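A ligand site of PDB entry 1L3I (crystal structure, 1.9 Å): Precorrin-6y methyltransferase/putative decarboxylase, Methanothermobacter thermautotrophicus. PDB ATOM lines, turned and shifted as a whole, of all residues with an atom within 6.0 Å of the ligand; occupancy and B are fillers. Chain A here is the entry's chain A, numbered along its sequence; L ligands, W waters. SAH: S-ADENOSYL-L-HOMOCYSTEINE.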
ATOM      1  N   VAL A  13      20.322  19.021   9.472  1.00  0.00           N
ATOM      2  CA  VAL A  13      21.077  18.597   8.303  1.00  0.00           C
ATOM      3  C   VAL A  13      22.516  19.127   8.413  1.00  0.00           C
ATOM      4  O   VAL A  13      22.732  20.332   8.559  1.00  0.00           O
ATOM      5  CB  VAL A  13      20.413  19.100   6.978  1.00  0.00           C
ATOM      6  CG1 VAL A  13      21.217  18.661   5.777  1.00  0.00           C
ATOM      7  CG2 VAL A  13      18.988  18.580   6.851  1.00  0.00           C
ATOM      8  N   PRO A  14      23.511  18.213   8.423  1.00  0.00           N
ATOM      9  CA  PRO A  14      24.905  18.654   8.519  1.00  0.00           C
ATOM     10  C   PRO A  14      25.434  19.309   7.268  1.00  0.00           C
ATOM     11  O   PRO A  14      24.925  19.089   6.182  1.00  0.00           O
ATOM     12  CB  PRO A  14      25.641  17.361   8.872  1.00  0.00           C
ATOM     13  CG  PRO A  14      24.777  16.291   8.331  1.00  0.00           C
ATOM     14  CD  PRO A  14      23.393  16.757   8.614  1.00  0.00           C
ATOM     15  N   GLY A  15      26.394  20.202   7.457  1.00  0.00           N
ATOM     16  CA  GLY A  15      27.008  20.861   6.317  1.00  0.00           C
ATOM     17  C   GLY A  15      26.820  22.356   6.366  1.00  0.00           C
ATOM     18  O   GLY A  15      26.269  22.872   7.333  1.00  0.00           O
ATOM     19  N   PRO A  16      27.313  23.100   5.360  1.00  0.00           N
ATOM     20  CA  PRO A  16      27.971  22.531   4.177  1.00  0.00           C
ATOM     21  C   PRO A  16      29.377  22.090   4.538  1.00  0.00           C
ATOM     22  O   PRO A  16      29.917  22.479   5.559  1.00  0.00           O
ATOM     23  CB  PRO A  16      27.998  23.721   3.228  1.00  0.00           C
ATOM     24  CG  PRO A  16      28.234  24.879   4.168  1.00  0.00           C
ATOM     25  CD  PRO A  16      27.246  24.561   5.295  1.00  0.00           C
ATOM     26  N   THR A  17      29.935  21.223   3.707  1.00  0.00           N
ATOM     27  CA  THR A  17      31.295  20.729   3.908  1.00  0.00           C
ATOM     28  C   THR A  17      32.226  21.944   3.758  1.00  0.00           C
ATOM     29  O   THR A  17      31.970  22.836   2.941  1.00  0.00           O
ATOM     30  CB  THR A  17      31.656  19.630   2.878  1.00  0.00           C
ATOM     31  OG1 THR A  17      30.850  18.480   3.137  1.00  0.00           O
ATOM     32  CG2 THR A  17      33.129  19.256   2.964  1.00  0.00           C
ATOM     33  N   ALA A  18      33.226  22.023   4.638  1.00  0.00           N
ATOM     34  CA  ALA A  18      34.216  23.086   4.652  1.00  0.00           C
ATOM     35  C   ALA A  18      34.633  23.480   3.231  1.00  0.00           C
ATOM     36  O   ALA A  18      35.084  22.624   2.460  1.00  0.00           O
ATOM     37  CB  ALA A  18      35.432  22.614   5.431  1.00  0.00           C
ATOM     38  N   ARG A  22      35.682  21.267   0.035  1.00  0.00           N
ATOM     39  CA  ARG A  22      34.888  21.224  -1.201  1.00  0.00           C
ATOM     40  C   ARG A  22      35.770  21.627  -2.390  1.00  0.00           C
ATOM     41  O   ARG A  22      35.644  21.081  -3.487  1.00  0.00           O
ATOM     42  CB  ARG A  22      33.678  22.147  -1.088  1.00  0.00           C
ATOM     43  CG  ARG A  22      32.662  21.684  -0.082  1.00  0.00           C
ATOM     44  CD  ARG A  22      31.400  22.509  -0.127  1.00  0.00           C
ATOM     45  NE  ARG A  22      31.597  23.859   0.391  1.00  0.00           N
ATOM     46  CZ  ARG A  22      31.438  24.964  -0.337  1.00  0.00           C
ATOM     47  NH1 ARG A  22      31.085  24.912  -1.607  1.00  0.00           N
ATOM     48  NH2 ARG A  22      31.673  26.156   0.214  1.00  0.00           N
ATOM     49  N   ASP A  39      25.963  12.673  -6.033  1.00  0.00           N
ATOM     50  CA  ASP A  39      26.381  13.122  -4.722  1.00  0.00           C
ATOM     51  C   ASP A  39      25.581  12.319  -3.713  1.00  0.00           C
ATOM     52  O   ASP A  39      24.397  12.597  -3.481  1.00  0.00           O
ATOM     53  CB  ASP A  39      26.146  14.626  -4.560  1.00  0.00           C
ATOM     54  CG  ASP A  39      26.620  15.173  -3.208  1.00  0.00           C
ATOM     55  OD1 ASP A  39      27.442  14.527  -2.542  1.00  0.00           O
ATOM     56  OD2 ASP A  39      26.170  16.254  -2.809  1.00  0.00           O
ATOM     57  N   VAL A  40      26.202  11.283  -3.153  1.00  0.00           N
ATOM     58  CA  VAL A  40      25.551  10.429  -2.177  1.00  0.00           C
ATOM     59  C   VAL A  40      25.577  11.112  -0.812  1.00  0.00           C
ATOM     60  O   VAL A  40      26.656  11.279  -0.215  1.00  0.00           O
ATOM     61  CB  VAL A  40      26.234   9.045  -2.105  1.00  0.00           C
ATOM     62  CG1 VAL A  40      25.564   8.154  -1.097  1.00  0.00           C
ATOM     63  CG2 VAL A  40      26.235   8.385  -3.475  1.00  0.00           C
ATOM     64  N   GLY A  41      24.398  11.497  -0.310  1.00  0.00           N
ATOM     65  CA  GLY A  41      24.319  12.167   0.969  1.00  0.00           C
ATOM     66  C   GLY A  41      24.607  13.626   0.725  1.00  0.00           C
ATOM     67  O   GLY A  41      25.596  14.157   1.198  1.00  0.00           O
ATOM     68  N   CYS A  42      23.718  14.292  -0.006  1.00  0.00           N
ATOM     69  CA  CYS A  42      23.927  15.699  -0.328  1.00  0.00           C
ATOM     70  C   CYS A  42      23.851  16.696   0.833  1.00  0.00           C
ATOM     71  O   CYS A  42      24.353  17.818   0.695  1.00  0.00           O
ATOM     72  CB  CYS A  42      23.043  16.142  -1.489  1.00  0.00           C
ATOM     73  SG  CYS A  42      21.289  15.984  -1.263  1.00  0.00           S
ATOM     74  N   GLY A  43      23.256  16.291   1.950  1.00  0.00           N
ATOM     75  CA  GLY A  43      23.136  17.156   3.122  1.00  0.00           C
ATOM     76  C   GLY A  43      22.611  18.556   2.829  1.00  0.00           C
ATOM     77  O   GLY A  43      21.512  18.697   2.318  1.00  0.00           O
ATOM     78  N   THR A  44      23.399  19.572   3.189  1.00  0.00           N
ATOM     79  CA  THR A  44      23.061  20.972   2.970  1.00  0.00           C
ATOM     80  C   THR A  44      23.205  21.384   1.480  1.00  0.00           C
ATOM     81  O   THR A  44      22.628  22.390   1.052  1.00  0.00           O
ATOM     82  CB  THR A  44      23.940  21.877   3.856  1.00  0.00           C
ATOM     83  OG1 THR A  44      23.741  21.519   5.225  1.00  0.00           O
ATOM     84  CG2 THR A  44      23.600  23.340   3.696  1.00  0.00           C
ATOM     85  N   GLY A  45      23.984  20.630   0.720  1.00  0.00           N
ATOM     86  CA  GLY A  45      24.151  20.935  -0.689  1.00  0.00           C
ATOM     87  C   GLY A  45      25.508  21.472  -1.083  1.00  0.00           C
ATOM     88  O   GLY A  45      25.724  21.800  -2.243  1.00  0.00           O
ATOM     89  N   GLY A  46      26.442  21.519  -0.148  1.00  0.00           N
ATOM     90  CA  GLY A  46      27.769  22.036  -0.435  1.00  0.00           C
ATOM     91  C   GLY A  46      28.463  21.440  -1.663  1.00  0.00           C
ATOM     92  O   GLY A  46      29.051  22.153  -2.462  1.00  0.00           O
ATOM     93  N   VAL A  47      28.416  20.115  -1.804  1.00  0.00           N
ATOM     94  CA  VAL A  47      29.053  19.461  -2.945  1.00  0.00           C
ATOM     95  C   VAL A  47      28.165  19.514  -4.187  1.00  0.00           C
ATOM     96  O   VAL A  47      28.647  19.760  -5.287  1.00  0.00           O
ATOM     97  CB  VAL A  47      29.440  18.013  -2.582  1.00  0.00           C
ATOM     98  CG1 VAL A  47      30.020  17.287  -3.772  1.00  0.00           C
ATOM     99  CG2 VAL A  47      30.446  18.014  -1.433  1.00  0.00           C
ATOM    100  N   ILE A  61      21.405  12.546  -3.701  1.00  0.00           N
ATOM    101  CA  ILE A  61      20.647  11.611  -2.888  1.00  0.00           C
ATOM    102  C   ILE A  61      20.773  11.888  -1.392  1.00  0.00           C
ATOM    103  O   ILE A  61      21.843  12.311  -0.925  1.00  0.00           O
ATOM    104  CB  ILE A  61      21.185  10.184  -3.107  1.00  0.00           C
ATOM    105  CG1 ILE A  61      21.139   9.815  -4.583  1.00  0.00           C
ATOM    106  CG2 ILE A  61      20.446   9.175  -2.272  1.00  0.00           C
ATOM    107  CD1 ILE A  61      21.937   8.564  -4.916  1.00  0.00           C
ATOM    108  N   ASP A  62      19.695  11.645  -0.645  1.00  0.00           N
ATOM    109  CA  ASP A  62      19.696  11.798   0.815  1.00  0.00           C
ATOM    110  C   ASP A  62      18.492  11.130   1.489  1.00  0.00           C
ATOM    111  O   ASP A  62      17.376  11.192   0.994  1.00  0.00           O
ATOM    112  CB  ASP A  62      19.768  13.269   1.224  1.00  0.00           C
ATOM    113  CG  ASP A  62      20.483  13.460   2.550  1.00  0.00           C
ATOM    114  OD1 ASP A  62      19.973  12.950   3.573  1.00  0.00           O
ATOM    115  OD2 ASP A  62      21.550  14.094   2.552  1.00  0.00           O
ATOM    116  N   ARG A  63      18.762  10.459   2.606  1.00  0.00           N
ATOM    117  CA  ARG A  63      17.745   9.794   3.414  1.00  0.00           C
ATOM    118  C   ARG A  63      16.815  10.851   4.011  1.00  0.00           C
ATOM    119  O   ARG A  63      15.602  10.653   4.106  1.00  0.00           O
ATOM    120  CB  ARG A  63      18.379   9.098   4.628  1.00  0.00           C
ATOM    121  CG  ARG A  63      19.262   7.926   4.386  1.00  0.00           C
ATOM    122  CD  ARG A  63      19.810   7.445   5.712  1.00  0.00           C
ATOM    123  NE  ARG A  63      20.617   6.239   5.546  1.00  0.00           N
ATOM    124  CZ  ARG A  63      20.949   5.415   6.540  1.00  0.00           C
ATOM    125  NH1 ARG A  63      20.546   5.633   7.773  1.00  0.00           N
ATOM    126  NH2 ARG A  63      21.702   4.348   6.281  1.00  0.00           N
ATOM    127  N   ASN A  64      17.436  11.922   4.491  1.00  0.00           N
ATOM    128  CA  ASN A  64      16.724  13.004   5.143  1.00  0.00           C
ATOM    129  C   ASN A  64      15.935  13.899   4.197  1.00  0.00           C
ATOM    130  O   ASN A  64      16.522  14.590   3.355  1.00  0.00           O
ATOM    131  CB  ASN A  64      17.703  13.853   5.972  1.00  0.00           C
ATOM    132  CG  ASN A  64      17.007  14.775   6.986  1.00  0.00           C
ATOM    133  OD1 ASN A  64      17.640  15.673   7.550  1.00  0.00           O
ATOM    134  ND2 ASN A  64      15.725  14.549   7.240  1.00  0.00           N
ATOM    135  N   ALA A  67      17.183  17.227   4.247  1.00  0.00           N
ATOM    136  CA  ALA A  67      18.431  17.479   3.537  1.00  0.00           C
ATOM    137  C   ALA A  67      18.078  17.772   2.064  1.00  0.00           C
ATOM    138  O   ALA A  67      18.643  18.671   1.439  1.00  0.00           O
ATOM    139  CB  ALA A  67      19.338  16.270   3.622  1.00  0.00           C
ATOM    140  N   GLY A  89      15.704   9.214  -0.246  1.00  0.00           N
ATOM    141  CA  GLY A  89      15.723   7.779  -0.042  1.00  0.00           C
ATOM    142  C   GLY A  89      17.099   7.280   0.329  1.00  0.00           C
ATOM    143  O   GLY A  89      18.083   8.014   0.291  1.00  0.00           O
ATOM    144  N   ASP A  90      17.145   6.005   0.680  1.00  0.00           N
ATOM    145  CA  ASP A  90      18.389   5.371   1.056  1.00  0.00           C
ATOM    146  C   ASP A  90      19.226   5.209  -0.220  1.00  0.00           C
ATOM    147  O   ASP A  90      18.707   4.816  -1.262  1.00  0.00           O
ATOM    148  CB  ASP A  90      18.073   4.010   1.688  1.00  0.00           C
ATOM    149  CG  ASP A  90      19.208   3.477   2.528  1.00  0.00           C
ATOM    150  OD1 ASP A  90      19.779   4.255   3.341  1.00  0.00           O
ATOM    151  OD2 ASP A  90      19.511   2.281   2.387  1.00  0.00           O
ATOM    152  N   ALA A  91      20.511   5.530  -0.127  1.00  0.00           N
ATOM    153  CA  ALA A  91      21.434   5.486  -1.257  1.00  0.00           C
ATOM    154  C   ALA A  91      21.463   4.272  -2.176  1.00  0.00           C
ATOM    155  O   ALA A  91      21.367   4.434  -3.390  1.00  0.00           O
ATOM    156  CB  ALA A  91      22.848   5.821  -0.793  1.00  0.00           C
ATOM    157  N   PRO A  92      21.634   3.054  -1.622  1.00  0.00           N
ATOM    158  CA  PRO A  92      21.678   1.900  -2.539  1.00  0.00           C
ATOM    159  C   PRO A  92      20.462   1.782  -3.470  1.00  0.00           C
ATOM    160  O   PRO A  92      20.631   1.638  -4.680  1.00  0.00           O
ATOM    161  CB  PRO A  92      21.827   0.729  -1.593  1.00  0.00           C
ATOM    162  CG  PRO A  92      22.632   1.335  -0.461  1.00  0.00           C
ATOM    163  CD  PRO A  92      21.860   2.611  -0.243  1.00  0.00           C
ATOM    164  N   GLY A 107      29.234  11.726   0.346  1.00  0.00           N
ATOM    165  CA  GLY A 107      29.269  12.659   1.464  1.00  0.00           C
ATOM    166  C   GLY A 107      28.742  12.089   2.772  1.00  0.00           C
ATOM    167  O   GLY A 107      28.895  12.731   3.817  1.00  0.00           O
ATOM    168  N   GLY A 108      28.112  10.920   2.716  1.00  0.00           N
ATOM    169  CA  GLY A 108      27.561  10.244   3.884  1.00  0.00           C
ATOM    170  C   GLY A 108      27.194   8.819   3.498  1.00  0.00           C
ATOM    171  O   GLY A 108      26.709   8.581   2.397  1.00  0.00           O
ATOM    172  N   SER A 109      27.468   7.856   4.367  1.00  0.00           N
ATOM    173  CA  SER A 109      27.150   6.455   4.046  1.00  0.00           C
ATOM    174  C   SER A 109      26.123   5.796   4.995  1.00  0.00           C
ATOM    175  O   SER A 109      25.492   4.807   4.636  1.00  0.00           O
ATOM    176  CB  SER A 109      28.440   5.645   3.966  1.00  0.00           C
ATOM    177  OG  SER A 109      29.176   5.745   5.185  1.00  0.00           O
ATOM    178  N   GLY A 110      26.020   6.321   6.220  1.00  0.00           N
ATOM    179  CA  GLY A 110      25.053   5.812   7.185  1.00  0.00           C
ATOM    180  C   GLY A 110      25.092   4.332   7.499  1.00  0.00           C
ATOM    181  O   GLY A 110      24.056   3.715   7.756  1.00  0.00           O
ATOM    182  N   GLY A 111      26.286   3.744   7.487  1.00  0.00           N
ATOM    183  CA  GLY A 111      26.415   2.330   7.780  1.00  0.00           C
ATOM    184  C   GLY A 111      26.447   1.444   6.559  1.00  0.00           C
ATOM    185  O   GLY A 111      26.827   0.293   6.662  1.00  0.00           O
ATOM    186  N   GLU A 112      26.105   2.001   5.402  1.00  0.00           N
ATOM    187  CA  GLU A 112      26.073   1.223   4.160  1.00  0.00           C
ATOM    188  C   GLU A 112      27.199   1.575   3.182  1.00  0.00           C
ATOM    189  O   GLU A 112      27.049   1.366   1.980  1.00  0.00           O
ATOM    190  CB  GLU A 112      24.727   1.429   3.464  1.00  0.00           C
ATOM    191  CG  GLU A 112      23.539   1.153   4.370  1.00  0.00           C
ATOM    192  CD  GLU A 112      22.230   1.643   3.787  1.00  0.00           C
ATOM    193  OE1 GLU A 112      22.252   2.549   2.929  1.00  0.00           O
ATOM    194  OE2 GLU A 112      21.176   1.111   4.202  1.00  0.00           O
ATOM    195  N   ILE A 116      27.212   0.826  -0.868  1.00  0.00           N
ATOM    196  CA  ILE A 116      27.183   2.043  -1.672  1.00  0.00           C
ATOM    197  C   ILE A 116      28.350   2.037  -2.643  1.00  0.00           C
ATOM    198  O   ILE A 116      28.168   2.313  -3.828  1.00  0.00           O
ATOM    199  CB  ILE A 116      27.271   3.298  -0.768  1.00  0.00           C
ATOM    200  CG1 ILE A 116      25.981   3.470   0.025  1.00  0.00           C
ATOM    201  CG2 ILE A 116      27.575   4.560  -1.574  1.00  0.00           C
ATOM    202  CD1 ILE A 116      26.075   4.574   1.062  1.00  0.00           C
HETATM  203  N   SAH L   1      28.505  17.267   1.859  1.00  0.00           N
HETATM  204  CA  SAH L   1      27.271  17.914   2.284  1.00  0.00           C
HETATM  205  CB  SAH L   1      26.842  17.468   3.705  1.00  0.00           C
HETATM  206  CG  SAH L   1      26.591  15.931   3.811  1.00  0.00           C
HETATM  207  SD  SAH L   1      26.055  15.317   5.409  1.00  0.00           S
HETATM  208  C   SAH L   1      27.456  19.419   2.234  1.00  0.00           C
HETATM  209  O   SAH L   1      28.559  19.846   1.852  1.00  0.00           O
HETATM  210  OXT SAH L   1      26.503  20.158   2.556  1.00  0.00           O
HETATM  211  C5' SAH L   1      25.837  13.579   5.081  1.00  0.00           C
HETATM  212  C4' SAH L   1      24.500  13.249   4.520  1.00  0.00           C
HETATM  213  O4' SAH L   1      24.523  11.826   4.359  1.00  0.00           O
HETATM  214  C3' SAH L   1      23.228  13.590   5.446  1.00  0.00           C
HETATM  215  O3' SAH L   1      22.274  14.586   4.977  1.00  0.00           O
HETATM  216  C2' SAH L   1      22.658  12.165   5.624  1.00  0.00           C
HETATM  217  O2' SAH L   1      21.244  12.039   5.875  1.00  0.00           O
HETATM  218  C1' SAH L   1      23.159  11.483   4.381  1.00  0.00           C
HETATM  219  N9  SAH L   1      23.219  10.034   4.315  1.00  0.00           N
HETATM  220  C8  SAH L   1      23.927   9.159   5.179  1.00  0.00           C
HETATM  221  N7  SAH L   1      23.770   7.919   4.835  1.00  0.00           N
HETATM  222  C5  SAH L   1      22.919   7.941   3.702  1.00  0.00           C
HETATM  223  C6  SAH L   1      22.378   6.941   2.884  1.00  0.00           C
HETATM  224  N6  SAH L   1      22.642   5.644   3.073  1.00  0.00           N
HETATM  225  N1  SAH L   1      21.571   7.293   1.846  1.00  0.00           N
HETATM  226  C2  SAH L   1      21.324   8.592   1.660  1.00  0.00           C
HETATM  227  N3  SAH L   1      21.770   9.617   2.367  1.00  0.00           N
HETATM  228  C4  SAH L   1      22.566   9.242   3.382  1.00  0.00           C
HETATM  229  O   HOH W   1      30.229  15.501   3.560  1.00  0.00           O
HETATM  230  O   HOH W   2      25.139  10.816   7.821  1.00  0.00           O
HETATM  231  O   HOH W   3      31.383  15.840   0.970  1.00  0.00           O
HETATM  232  O   HOH W   4      27.899  15.366  -0.133  1.00  0.00           O
HETATM  233  O   HOH W   5      20.077  10.566   7.647  1.00  0.00           O
HETATM  234  O   HOH W   6      20.870  14.968   7.269  1.00  0.00           O
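An oxygen (O3') of the ligand lies within hydrogen-bond range of the side-chain carboxylate (OD2) of Asp 62 (2.6 Å). The backbone NH (N) of Thr 17 is in hydrogen-bond range of an oxygen (O) of the ligand (2.7 Å). A nitrogen (N) of the ligand sits at hydrogen-bond distance from the side-chain hydroxyl (OG1) of Thr 17. N of Ala 91 is in hydrogen-bond range of N1 of the ligand (2.9 Å). The backbone NH of Gly 46 is in hydrogen-bond range of an oxygen (OXT) of the ligand (3.0 Å). N of Gly 110 is in hydrogen-bond range of N7 of the ligand (3.1 Å). OE1 of Glu 112 is in hydrogen-bond range of N6 of the ligand. N of Arg 63 is in hydrogen-bond range of N3 of the ligand (3.1 Å). OXT of the ligand sits at hydrogen-bond distance from N of Gly 45 (3.2 Å). N6 of the ligand lies within hydrogen-bond range of O of Ser 109 (3.4 Å). The side-chain carboxylate (OD1) of Asp 90 is in hydrogen-bond range of a nitrogen (N6) of the ligand, at 3.2 Å. An oxygen (OXT) of the ligand sits at hydrogen-bond distance from the backbone NH (N) of Thr 44.
Merely in contact with the ligand: Pro 16 (3.2 Å), Gly 43 (3.3 Å), Gly 41 (3.3 Å), Cys 42 (3.3 Å), Pro 14 (3.3 Å), Gly 107 (3.4 Å), Gly 108 (3.5 Å), Gly 89 (3.6 Å), Ala 67 (3.6 Å), Val 47 (3.7 Å), Gly 15 (3.9 Å) and Asn 64 (3.98 Å). Hydrophobic or aromatic side chains within 4 Å of the ligand: Pro 14, Pro 16, Val 47, Ala 67 and Ala 91. Within 4 Å of the ligand: Pro 14, Gly 15, Pro 16, Thr 17, Gly 41, Cys 42, Gly 43, Thr 44, Gly 45, Gly 46, Val 47, Asp 62, Arg 63, Asn 64, Ala 67, Gly 89, Asp 90, Ala 91, Gly 107, Gly 108, Ser 109, Gly 110 and Glu 112. The nearest printed residue that does not touch the ligand is Ile 61 (4.1 Å).
Water W6 bridges an oxygen (O3') of the ligand (2.7 Å) and the side-chain amide oxygen (OD1) of Asn 64 (3.3 Å). Water W4 lies within hydrogen-bond range of OD1 of Asp 39 (2.6 Å), N of the ligand (2.8 Å) and O of Gly 41 (2.9 Å). Water W1 lies within hydrogen-bond range of a nitrogen (N) of the ligand (3.0 Å), the side-chain hydroxyl of Thr 17 (3.1 Å) and the backbone carbonyl oxygen of Gly 107 (3.1 Å). Water W3 bridges a nitrogen (N) of the ligand and the side-chain hydroxyl (OG1) of Thr 17.
N of Gly 43 lies within hydrogen-bond range of OD2 of Asp 62. The side-chain carboxylate of Asp 62 is in hydrogen-bond range of the backbone NH of Cys 42, 3.4 Å away. The backbone NH (N) of Gly 89 sits at hydrogen-bond distance from the backbone carbonyl oxygen (O) of Asp 62 (2.9 Å). OD1 of Asp 62 lies within hydrogen-bond range of N of Asn 64 (2.9 Å). NH2 of Arg 63 is in salt-bridge range of OE1 of Glu 112, 3.8 Å away. OE2 of Glu 112 sits close to OD2 of Asp 90, 2.7 Å away. The backbone carbonyl oxygen (O) of Gly 89 sits at hydrogen-bond distance from the backbone NH (N) of Arg 63, 3.4 Å away. N of Gly 108 lies within hydrogen-bond range of O of Val 40, at 3.3 Å.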
